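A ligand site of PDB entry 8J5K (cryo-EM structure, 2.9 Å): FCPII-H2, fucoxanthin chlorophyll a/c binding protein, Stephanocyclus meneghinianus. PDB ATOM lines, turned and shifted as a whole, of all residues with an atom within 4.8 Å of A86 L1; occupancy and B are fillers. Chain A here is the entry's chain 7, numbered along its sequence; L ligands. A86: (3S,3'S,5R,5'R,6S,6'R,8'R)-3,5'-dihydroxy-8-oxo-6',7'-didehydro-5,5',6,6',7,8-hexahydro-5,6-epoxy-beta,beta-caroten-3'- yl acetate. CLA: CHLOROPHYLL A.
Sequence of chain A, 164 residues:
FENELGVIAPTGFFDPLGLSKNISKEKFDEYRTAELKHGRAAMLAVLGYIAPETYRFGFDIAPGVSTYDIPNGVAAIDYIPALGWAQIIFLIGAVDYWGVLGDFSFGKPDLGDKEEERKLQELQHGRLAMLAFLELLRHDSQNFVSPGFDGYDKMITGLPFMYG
NE2 of Gln 124 lies close to O2 of A86 L1, 3.4 Å away.
O2 of A86 L1 lies within hydrogen-bond range of O of Pro 10 (2.9 Å).
NH2 of Arg 127 sits at hydrogen-bond distance from O1D of CLA L3, at 3.0 Å.
The side-chain amide oxygen (OE1) of Gln 124 sits at hydrogen-bond distance from the guanidinium group (NH1) of Arg 127, 3.0 Å away.
Residues that only touch A86 L1: Leu 131 and Leu 128.
Hydrophobic or aromatic side chains within 4 Å of A86 L1: Pro 10 and Leu 131.
Within 4 Å of A86 L1: Pro 10, Gln 124, Leu 128 and Leu 131.
The nearest printed residue that does not touch A86 L1 is Arg 127 (4.02 Å).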
ATOM      1  N   PRO A  10      30.793  12.683   4.207  1.00  0.00           N
ATOM      2  CA  PRO A  10      31.268  13.290   2.958  1.00  0.00           C
ATOM      3  C   PRO A  10      30.242  14.301   2.484  1.00  0.00           C
ATOM      4  O   PRO A  10      29.126  13.890   2.135  1.00  0.00           O
ATOM      5  CB  PRO A  10      31.397  12.104   2.008  1.00  0.00           C
ATOM      6  CG  PRO A  10      30.352  11.159   2.473  1.00  0.00           C
ATOM      7  CD  PRO A  10      30.329  11.301   3.979  1.00  0.00           C
ATOM      8  N   THR A  11      30.568  15.593   2.483  1.00  0.00           N
ATOM      9  CA  THR A  11      29.571  16.597   2.148  1.00  0.00           C
ATOM     10  C   THR A  11      28.405  16.592   3.144  1.00  0.00           C
ATOM     11  O   THR A  11      27.396  15.909   2.915  1.00  0.00           O
ATOM     12  CB  THR A  11      29.054  16.407   0.720  1.00  0.00           C
ATOM     13  OG1 THR A  11      30.146  16.514  -0.198  1.00  0.00           O
ATOM     14  CG2 THR A  11      28.008  17.440   0.379  1.00  0.00           C
ATOM     15  N   GLN A 124      20.626   7.244   1.084  1.00  0.00           N
ATOM     16  CA  GLN A 124      21.943   7.271   0.470  1.00  0.00           C
ATOM     17  C   GLN A 124      22.050   6.259  -0.665  1.00  0.00           C
ATOM     18  O   GLN A 124      22.655   6.539  -1.713  1.00  0.00           O
ATOM     19  CB  GLN A 124      23.021   7.031   1.519  1.00  0.00           C
ATOM     20  CG  GLN A 124      24.378   7.565   1.119  1.00  0.00           C
ATOM     21  CD  GLN A 124      24.550   9.038   1.433  1.00  0.00           C
ATOM     22  OE1 GLN A 124      23.588   9.812   1.394  1.00  0.00           O
ATOM     23  NE2 GLN A 124      25.764   9.432   1.750  1.00  0.00           N
ATOM     24  N   ARG A 127      20.407   7.827  -3.587  1.00  0.00           N
ATOM     25  CA  ARG A 127      21.256   8.831  -4.198  1.00  0.00           C
ATOM     26  C   ARG A 127      22.301   8.201  -5.106  1.00  0.00           C
ATOM     27  O   ARG A 127      22.553   8.684  -6.211  1.00  0.00           O
ATOM     28  CB  ARG A 127      21.909   9.678  -3.108  1.00  0.00           C
ATOM     29  CG  ARG A 127      20.911  10.526  -2.362  1.00  0.00           C
ATOM     30  CD  ARG A 127      21.488  11.066  -1.076  1.00  0.00           C
ATOM     31  NE  ARG A 127      20.639  12.124  -0.537  1.00  0.00           N
ATOM     32  CZ  ARG A 127      20.749  12.607   0.692  1.00  0.00           C
ATOM     33  NH1 ARG A 127      21.669  12.160   1.539  1.00  0.00           N
ATOM     34  NH2 ARG A 127      19.920  13.562   1.091  1.00  0.00           N
ATOM     35  N   LEU A 128      22.922   7.104  -4.656  1.00  0.00           N
ATOM     36  CA  LEU A 128      23.883   6.424  -5.518  1.00  0.00           C
ATOM     37  C   LEU A 128      23.202   5.780  -6.728  1.00  0.00           C
ATOM     38  O   LEU A 128      23.721   5.837  -7.856  1.00  0.00           O
ATOM     39  CB  LEU A 128      24.663   5.385  -4.724  1.00  0.00           C
ATOM     40  CG  LEU A 128      25.602   4.506  -5.566  1.00  0.00           C
ATOM     41  CD1 LEU A 128      26.673   5.368  -6.213  1.00  0.00           C
ATOM     42  CD2 LEU A 128      26.220   3.419  -4.717  1.00  0.00           C
ATOM     43  N   LEU A 131      22.460   8.100  -9.811  1.00  0.00           N
ATOM     44  CA  LEU A 131      23.615   8.328 -10.677  1.00  0.00           C
ATOM     45  C   LEU A 131      23.951   7.071 -11.472  1.00  0.00           C
ATOM     46  O   LEU A 131      24.353   7.159 -12.650  1.00  0.00           O
ATOM     47  CB  LEU A 131      24.805   8.787  -9.844  1.00  0.00           C
ATOM     48  CG  LEU A 131      24.563  10.040  -9.019  1.00  0.00           C
ATOM     49  CD1 LEU A 131      25.832  10.481  -8.338  1.00  0.00           C
ATOM     50  CD2 LEU A 131      24.014  11.151  -9.893  1.00  0.00           C
HETATM   51  C   A86 L   1      30.480  16.570 -15.562  1.00  0.00           C
HETATM   52  O   A86 L   1      29.710   9.735  -4.659  1.00  0.00           O
HETATM   53  C1  A86 L   1      30.715  15.244 -16.215  1.00  0.00           C
HETATM   54  C10 A86 L   1      29.147  11.170  -7.601  1.00  0.00           C
HETATM   55  C11 A86 L   1      29.118  10.075  -6.843  1.00  0.00           C
HETATM   56  C12 A86 L   1      29.351   8.722  -7.449  1.00  0.00           C
HETATM   57  C13 A86 L   1      28.872  10.185  -5.413  1.00  0.00           C
HETATM   58  C14 A86 L   1      27.588  10.761  -4.853  1.00  0.00           C
HETATM   59  C15 A86 L   1      27.593  10.853  -3.326  1.00  0.00           C
HETATM   60  C16 A86 L   1      28.346  12.077  -2.748  1.00  0.00           C
HETATM   61  C17 A86 L   1      28.449  12.171  -1.226  1.00  0.00           C
HETATM   62  C18 A86 L   1      27.051  12.144  -0.683  1.00  0.00           C
HETATM   63  C19 A86 L   1      26.444  10.776  -0.974  1.00  0.00           C
HETATM   64  C2  A86 L   1      30.598  14.109 -15.511  1.00  0.00           C
HETATM   65  C20 A86 L   1      26.558  10.233  -2.394  1.00  0.00           C
HETATM   66  C21 A86 L   1      25.822   8.924  -2.602  1.00  0.00           C
HETATM   67  C22 A86 L   1      27.543  13.291  -3.219  1.00  0.00           C
HETATM   68  C23 A86 L   1      29.765  12.312  -3.236  1.00  0.00           C
HETATM   69  C24 A86 L   1      31.086  15.170 -17.636  1.00  0.00           C
HETATM   70  C25 A86 L   1      31.250  16.258 -18.372  1.00  0.00           C
HETATM   71  C26 A86 L   1      31.627  16.049 -19.759  1.00  0.00           C
HETATM   72  C27 A86 L   1      31.844  17.038 -20.650  1.00  0.00           C
HETATM   73  C28 A86 L   1      31.709  18.484 -20.290  1.00  0.00           C
HETATM   74  C29 A86 L   1      32.224  16.600 -22.005  1.00  0.00           C
HETATM   75  C3  A86 L   1      30.251  14.168 -14.099  1.00  0.00           C
HETATM   76  C30 A86 L   1      32.473  17.291 -23.029  1.00  0.00           C
HETATM   77  C31 A86 L   1      32.749  17.809 -24.133  1.00  0.00           C
HETATM   78  C32 A86 L   1      33.635  19.046 -24.190  1.00  0.00           C
HETATM   79  C33 A86 L   1      34.346  19.079 -25.547  1.00  0.00           C
HETATM   80  C34 A86 L   1      33.356  19.128 -26.728  1.00  0.00           C
HETATM   81  C35 A86 L   1      32.672  17.790 -26.549  1.00  0.00           C
HETATM   82  C36 A86 L   1      31.853  17.478 -25.285  1.00  0.00           C
HETATM   83  C37 A86 L   1      30.511  18.210 -25.257  1.00  0.00           C
HETATM   84  C38 A86 L   1      33.076  21.527 -27.041  1.00  0.00           C
HETATM   85  C39 A86 L   1      32.661  22.267 -28.281  1.00  0.00           C
HETATM   86  C4  A86 L   1      30.160  13.049 -13.383  1.00  0.00           C
HETATM   87  C40 A86 L   1      32.799  20.282 -23.850  1.00  0.00           C
HETATM   88  C41 A86 L   1      34.698  18.893 -23.108  1.00  0.00           C
HETATM   89  C5  A86 L   1      29.835  13.130 -11.964  1.00  0.00           C
HETATM   90  C6  A86 L   1      29.765  12.019 -11.222  1.00  0.00           C
HETATM   91  C7  A86 L   1      30.004  10.675 -11.842  1.00  0.00           C
HETATM   92  C8  A86 L   1      29.466  12.133  -9.787  1.00  0.00           C
HETATM   93  C9  A86 L   1      29.423  11.038  -9.034  1.00  0.00           C
HETATM   94  O1  A86 L   1      26.174  11.171  -3.363  1.00  0.00           O
HETATM   95  O2  A86 L   1      27.097  12.334   0.728  1.00  0.00           O
HETATM   96  O3  A86 L   1      31.594  16.070 -25.253  1.00  0.00           O
HETATM   97  O4  A86 L   1      32.448  20.239 -26.777  1.00  0.00           O
HETATM   98  O5  A86 L   1      33.921  21.982 -26.289  1.00  0.00           O
HETATM   99 MG   CLA L   2      29.364   6.712   2.545  1.00  0.00          MG
HETATM  100  CHA CLA L   2      26.913   5.027   4.339  1.00  0.00           C
HETATM  101  CHB CLA L   2      30.880   7.589   5.468  1.00  0.00           C
HETATM  102  CHC CLA L   2      31.832   8.260   0.731  1.00  0.00           C
HETATM  103  CHD CLA L   2      27.838   5.645  -0.460  1.00  0.00           C
HETATM  104  NA  CLA L   2      28.925   6.377   4.561  1.00  0.00           N
HETATM  105  C1A CLA L   2      27.861   5.644   5.112  1.00  0.00           C
HETATM  106  C2A CLA L   2      27.937   5.644   6.637  1.00  0.00           C
HETATM  107  C3A CLA L   2      29.184   6.485   6.954  1.00  0.00           C
HETATM  108  C4A CLA L   2      29.716   6.860   5.571  1.00  0.00           C
HETATM  109  CMA CLA L   2      28.902   7.667   7.848  1.00  0.00           C
HETATM  110  CAA CLA L   2      28.149   4.231   7.162  1.00  0.00           C
HETATM  111  NB  CLA L   2      31.040   7.735   3.008  1.00  0.00           N
HETATM  112  C1B CLA L   2      31.492   7.992   4.257  1.00  0.00           C
HETATM  113  C2B CLA L   2      32.763   8.751   4.194  1.00  0.00           C
HETATM  114  C3B CLA L   2      33.043   8.948   2.856  1.00  0.00           C
HETATM  115  C4B CLA L   2      31.951   8.303   2.086  1.00  0.00           C
HETATM  116  CMB CLA L   2      33.512   9.173   5.372  1.00  0.00           C
HETATM  117  CAB CLA L   2      34.153   9.632   2.249  1.00  0.00           C
HETATM  118  CBB CLA L   2      34.970   9.130   1.325  1.00  0.00           C
HETATM  119  NC  CLA L   2      29.731   6.943   0.512  1.00  0.00           N
HETATM  120  C1C CLA L   2      30.794   7.631  -0.018  1.00  0.00           C
HETATM  121  C2C CLA L   2      30.752   7.595  -1.469  1.00  0.00           C
HETATM  122  C3C CLA L   2      29.633   6.830  -1.807  1.00  0.00           C
HETATM  123  C4C CLA L   2      29.004   6.421  -0.564  1.00  0.00           C
HETATM  124  CMC CLA L   2      31.720   8.239  -2.353  1.00  0.00           C
HETATM  125  CAC CLA L   2      29.169   6.499  -3.161  1.00  0.00           C
HETATM  126  CBC CLA L   2      29.461   5.062  -3.523  1.00  0.00           C
HETATM  127  ND  CLA L   2      27.725   5.682   1.992  1.00  0.00           N
HETATM  128  C1D CLA L   2      27.231   5.282   0.720  1.00  0.00           C
HETATM  129  C2D CLA L   2      26.006   4.478   0.912  1.00  0.00           C
HETATM  130  C3D CLA L   2      25.833   4.373   2.273  1.00  0.00           C
HETATM  131  C4D CLA L   2      26.935   5.106   2.910  1.00  0.00           C
HETATM  132  CMD CLA L   2      25.201   3.938  -0.180  1.00  0.00           C
HETATM  133  CAD CLA L   2      25.004   3.845   3.339  1.00  0.00           C
HETATM  134  OBD CLA L   2      23.926   3.251   3.287  1.00  0.00           O
HETATM  135  CBD CLA L   2      25.712   4.172   4.677  1.00  0.00           C
HETATM  136  CGD CLA L   2      24.728   4.823   5.605  1.00  0.00           C
HETATM  137  O1D CLA L   2      23.641   5.326   5.303  1.00  0.00           O
HETATM  138  O2D CLA L   2      25.074   4.831   6.920  1.00  0.00           O
HETATM  139  CED CLA L   2      24.423   5.765   7.776  1.00  0.00           C
HETATM  140 MG   CLA L   3      19.100  15.317  -2.825  1.00  0.00          MG
HETATM  141  CHA CLA L   3      19.659  16.925   0.197  1.00  0.00           C
HETATM  142  CHB CLA L   3      15.952  16.593  -2.925  1.00  0.00           C
HETATM  143  CHC CLA L   3      18.652  13.805  -5.883  1.00  0.00           C
HETATM  144  CHD CLA L   3      22.362  13.965  -2.654  1.00  0.00           C
HETATM  145  NA  CLA L   3      18.003  16.553  -1.549  1.00  0.00           N
HETATM  146  C1A CLA L   3      18.421  17.127  -0.340  1.00  0.00           C
HETATM  147  C2A CLA L   3      17.303  17.969   0.269  1.00  0.00           C
HETATM  148  C3A CLA L   3      16.103  17.755  -0.687  1.00  0.00           C
HETATM  149  C4A CLA L   3      16.711  16.915  -1.811  1.00  0.00           C
HETATM  150  CMA CLA L   3      14.962  17.051  -0.012  1.00  0.00           C
HETATM  151  CAA CLA L   3      17.679  19.444   0.297  1.00  0.00           C
HETATM  152  CBA CLA L   3      18.481  19.830  -0.928  1.00  0.00           C
HETATM  153  CGA CLA L   3      17.578  20.213  -2.062  1.00  0.00           C
HETATM  154  O1A CLA L   3      17.285  19.580  -3.066  1.00  0.00           O
HETATM  155  O2A CLA L   3      17.028  21.456  -1.892  1.00  0.00           O
HETATM  156  NB  CLA L   3      17.580  15.203  -4.136  1.00  0.00           N
HETATM  157  C1B CLA L   3      16.378  15.812  -4.006  1.00  0.00           C
HETATM  158  C2B CLA L   3      15.548  15.540  -5.213  1.00  0.00           C
HETATM  159  C3B CLA L   3      16.297  14.758  -6.055  1.00  0.00           C
HETATM  160  C4B CLA L   3      17.608  14.526  -5.378  1.00  0.00           C
HETATM  161  CMB CLA L   3      14.191  16.076  -5.371  1.00  0.00           C
HETATM  162  CAB CLA L   3      15.982  14.207  -7.348  1.00  0.00           C
HETATM  163  CBB CLA L   3      14.852  13.561  -7.633  1.00  0.00           C
HETATM  164  NC  CLA L   3      20.297  14.119  -4.043  1.00  0.00           N
HETATM  165  C1C CLA L   3      19.924  13.618  -5.263  1.00  0.00           C
HETATM  166  C2C CLA L   3      21.030  12.845  -5.828  1.00  0.00           C
HETATM  167  C3C CLA L   3      22.062  12.879  -4.904  1.00  0.00           C
HETATM  168  C4C CLA L   3      21.597  13.682  -3.789  1.00  0.00           C
HETATM  169  CMC CLA L   3      21.031  12.165  -7.123  1.00  0.00           C
HETATM  170  CAC CLA L   3      23.387  12.257  -5.048  1.00  0.00           C
HETATM  171  CBC CLA L   3      24.428  13.259  -5.474  1.00  0.00           C
HETATM  172  ND  CLA L   3      20.678  15.398  -1.584  1.00  0.00           N
HETATM  173  C1D CLA L   3      21.946  14.746  -1.604  1.00  0.00           C
HETATM  174  C2D CLA L   3      22.697  15.104  -0.394  1.00  0.00           C
HETATM  175  C3D CLA L   3      21.893  15.992   0.310  1.00  0.00           C
HETATM  176  C4D CLA L   3      20.639  16.109  -0.466  1.00  0.00           C
HETATM  177  CMD CLA L   3      24.039  14.601  -0.095  1.00  0.00           C
HETATM  178  CAD CLA L   3      21.756  16.819   1.492  1.00  0.00           C
HETATM  179  OBD CLA L   3      22.577  17.070   2.359  1.00  0.00           O
HETATM  180  CBD CLA L   3      20.310  17.386   1.476  1.00  0.00           C
HETATM  181  CGD CLA L   3      19.526  16.944   2.687  1.00  0.00           C
HETATM  182  O1D CLA L   3      18.978  15.855   2.867  1.00  0.00           O
HETATM  183  O2D CLA L   3      19.438  17.885   3.666  1.00  0.00           O
HETATM  184  CED CLA L   3      18.595  17.606   4.780  1.00  0.00           C
HETATM  185 MG   CLA L   4      24.927  12.311 -24.845  1.00  0.00          MG
HETATM  186  CHA CLA L   4      24.804  12.089 -28.308  1.00  0.00           C
HETATM  187  CHB CLA L   4      27.957  13.830 -25.052  1.00  0.00           C
HETATM  188  CHC CLA L   4      24.983  12.568 -21.421  1.00  0.00           C
HETATM  189  CHD CLA L   4      21.759  10.755 -24.674  1.00  0.00           C
HETATM  190  NA  CLA L   4      26.161  12.856 -26.443  1.00  0.00           N
HETATM  191  C1A CLA L   4      25.931  12.679 -27.812  1.00  0.00           C
HETATM  192  C2A CLA L   4      27.092  13.228 -28.637  1.00  0.00           C
HETATM  193  C3A CLA L   4      28.103  13.711 -27.571  1.00  0.00           C
HETATM  194  C4A CLA L   4      27.375  13.469 -26.255  1.00  0.00           C
HETATM  195  CMA CLA L   4      29.397  12.957 -27.636  1.00  0.00           C
HETATM  196  CAA CLA L   4      26.640  14.412 -29.482  1.00  0.00           C
HETATM  197  NB  CLA L   4      26.236  13.026 -23.500  1.00  0.00           N
HETATM  198  C1B CLA L   4      27.403  13.653 -23.784  1.00  0.00           C
HETATM  199  C2B CLA L   4      28.032  14.140 -22.525  1.00  0.00           C
HETATM  200  C3B CLA L   4      27.190  13.788 -21.491  1.00  0.00           C
HETATM  201  C4B CLA L   4      26.040  13.070 -22.093  1.00  0.00           C
HETATM  202  CMB CLA L   4      29.299  14.860 -22.535  1.00  0.00           C
HETATM  203  CAB CLA L   4      27.292  14.005 -20.065  1.00  0.00           C
HETATM  204  CBB CLA L   4      27.902  15.023 -19.463  1.00  0.00           C
HETATM  205  NC  CLA L   4      23.610  11.752 -23.335  1.00  0.00           N
HETATM  206  C1C CLA L   4      23.831  11.953 -22.004  1.00  0.00           C
HETATM  207  C2C CLA L   4      22.716  11.454 -21.224  1.00  0.00           C
HETATM  208  C3C CLA L   4      21.788  10.945 -22.136  1.00  0.00           C
HETATM  209  C4C CLA L   4      22.362  11.140 -23.464  1.00  0.00           C
HETATM  210  CMC CLA L   4      22.635  11.520 -19.756  1.00  0.00           C
HETATM  211  CAC CLA L   4      20.487  10.344 -21.848  1.00  0.00           C
HETATM  212  CBC CLA L   4      20.609   9.014 -21.172  1.00  0.00           C
HETATM  213  ND  CLA L   4      23.547  11.597 -26.131  1.00  0.00           N
HETATM  214  C1D CLA L   4      22.294  10.959 -25.926  1.00  0.00           C
HETATM  215  C2D CLA L   4      21.729  10.596 -27.250  1.00  0.00           C
HETATM  216  C3D CLA L   4      22.648  11.004 -28.195  1.00  0.00           C
HETATM  217  C4D CLA L   4      23.759  11.623 -27.441  1.00  0.00           C
HETATM  218  CMD CLA L   4      20.444   9.944 -27.451  1.00  0.00           C
HETATM  219  CAD CLA L   4      22.969  11.109 -29.603  1.00  0.00           C
HETATM  220  OBD CLA L   4      22.307  10.758 -30.581  1.00  0.00           O
HETATM  221  CBD CLA L   4      24.370  11.762 -29.712  1.00  0.00           C
HETATM  222  CGD CLA L   4      25.363  10.847 -30.380  1.00  0.00           C
HETATM  223 MG   CLA L   5      30.102   7.902 -16.159  1.00  0.00          MG
HETATM  224  CHA CLA L   5      32.432   7.215 -18.643  1.00  0.00           C
HETATM  225  CHB CLA L   5      30.875   4.969 -14.637  1.00  0.00           C
HETATM  226  CHC CLA L   5      27.803   8.643 -13.716  1.00  0.00           C
HETATM  227  CHD CLA L   5      29.286  10.909 -17.834  1.00  0.00           C
HETATM  228  NA  CLA L   5      31.447   6.363 -16.588  1.00  0.00           N
HETATM  229  C1A CLA L   5      32.338   6.256 -17.671  1.00  0.00           C
HETATM  230  C2A CLA L   5      33.143   4.968 -17.602  1.00  0.00           C
HETATM  231  C3A CLA L   5      32.556   4.243 -16.365  1.00  0.00           C
HETATM  232  C4A CLA L   5      31.564   5.260 -15.804  1.00  0.00           C
HETATM  233  CMA CLA L   5      31.860   2.963 -16.761  1.00  0.00           C
HETATM  234  CAA CLA L   5      34.613   5.255 -17.373  1.00  0.00           C
HETATM  235  NB  CLA L   5      29.439   6.971 -14.510  1.00  0.00           N
HETATM  236  C1B CLA L   5      29.932   5.799 -14.017  1.00  0.00           C
HETATM  237  C2B CLA L   5      29.303   5.510 -12.694  1.00  0.00           C
HETATM  238  C3B CLA L   5      28.431   6.542 -12.426  1.00  0.00           C
HETATM  239  C4B CLA L   5      28.509   7.488 -13.581  1.00  0.00           C
HETATM  240  CMB CLA L   5      29.645   4.314 -11.923  1.00  0.00           C
HETATM  241  CAB CLA L   5      27.558   6.791 -11.315  1.00  0.00           C
HETATM  242  CBB CLA L   5      27.097   5.884 -10.446  1.00  0.00           C
HETATM  243  NC  CLA L   5      28.785   9.492 -15.852  1.00  0.00           N
HETATM  244  C1C CLA L   5      27.928   9.586 -14.786  1.00  0.00           C
HETATM  245  C2C CLA L   5      27.151  10.820 -14.877  1.00  0.00           C
HETATM  246  C3C CLA L   5      27.565  11.464 -16.047  1.00  0.00           C
HETATM  247  C4C CLA L   5      28.597  10.619 -16.645  1.00  0.00           C
HETATM  248  CMC CLA L   5      26.138  11.234 -13.912  1.00  0.00           C
HETATM  249  ND  CLA L   5      30.702   8.913 -17.810  1.00  0.00           N
HETATM  250  C1D CLA L   5      30.272  10.127 -18.397  1.00  0.00           C
HETATM  251  C2D CLA L   5      31.036  10.363 -19.641  1.00  0.00           C
HETATM  252  C3D CLA L   5      31.893   9.283 -19.774  1.00  0.00           C
HETATM  253  C4D CLA L   5      31.625   8.400 -18.626  1.00  0.00           C
HETATM  254  CMD CLA L   5      30.886  11.533 -20.501  1.00  0.00           C
HETATM  255  CAD CLA L   5      32.931   8.657 -20.569  1.00  0.00           C
HETATM  256  OBD CLA L   5      33.488   9.066 -21.591  1.00  0.00           O
HETATM  257  CBD CLA L   5      33.270   7.291 -19.901  1.00  0.00           C
HETATM  258  CGD CLA L   5      32.992   6.141 -20.832  1.00  0.00           C
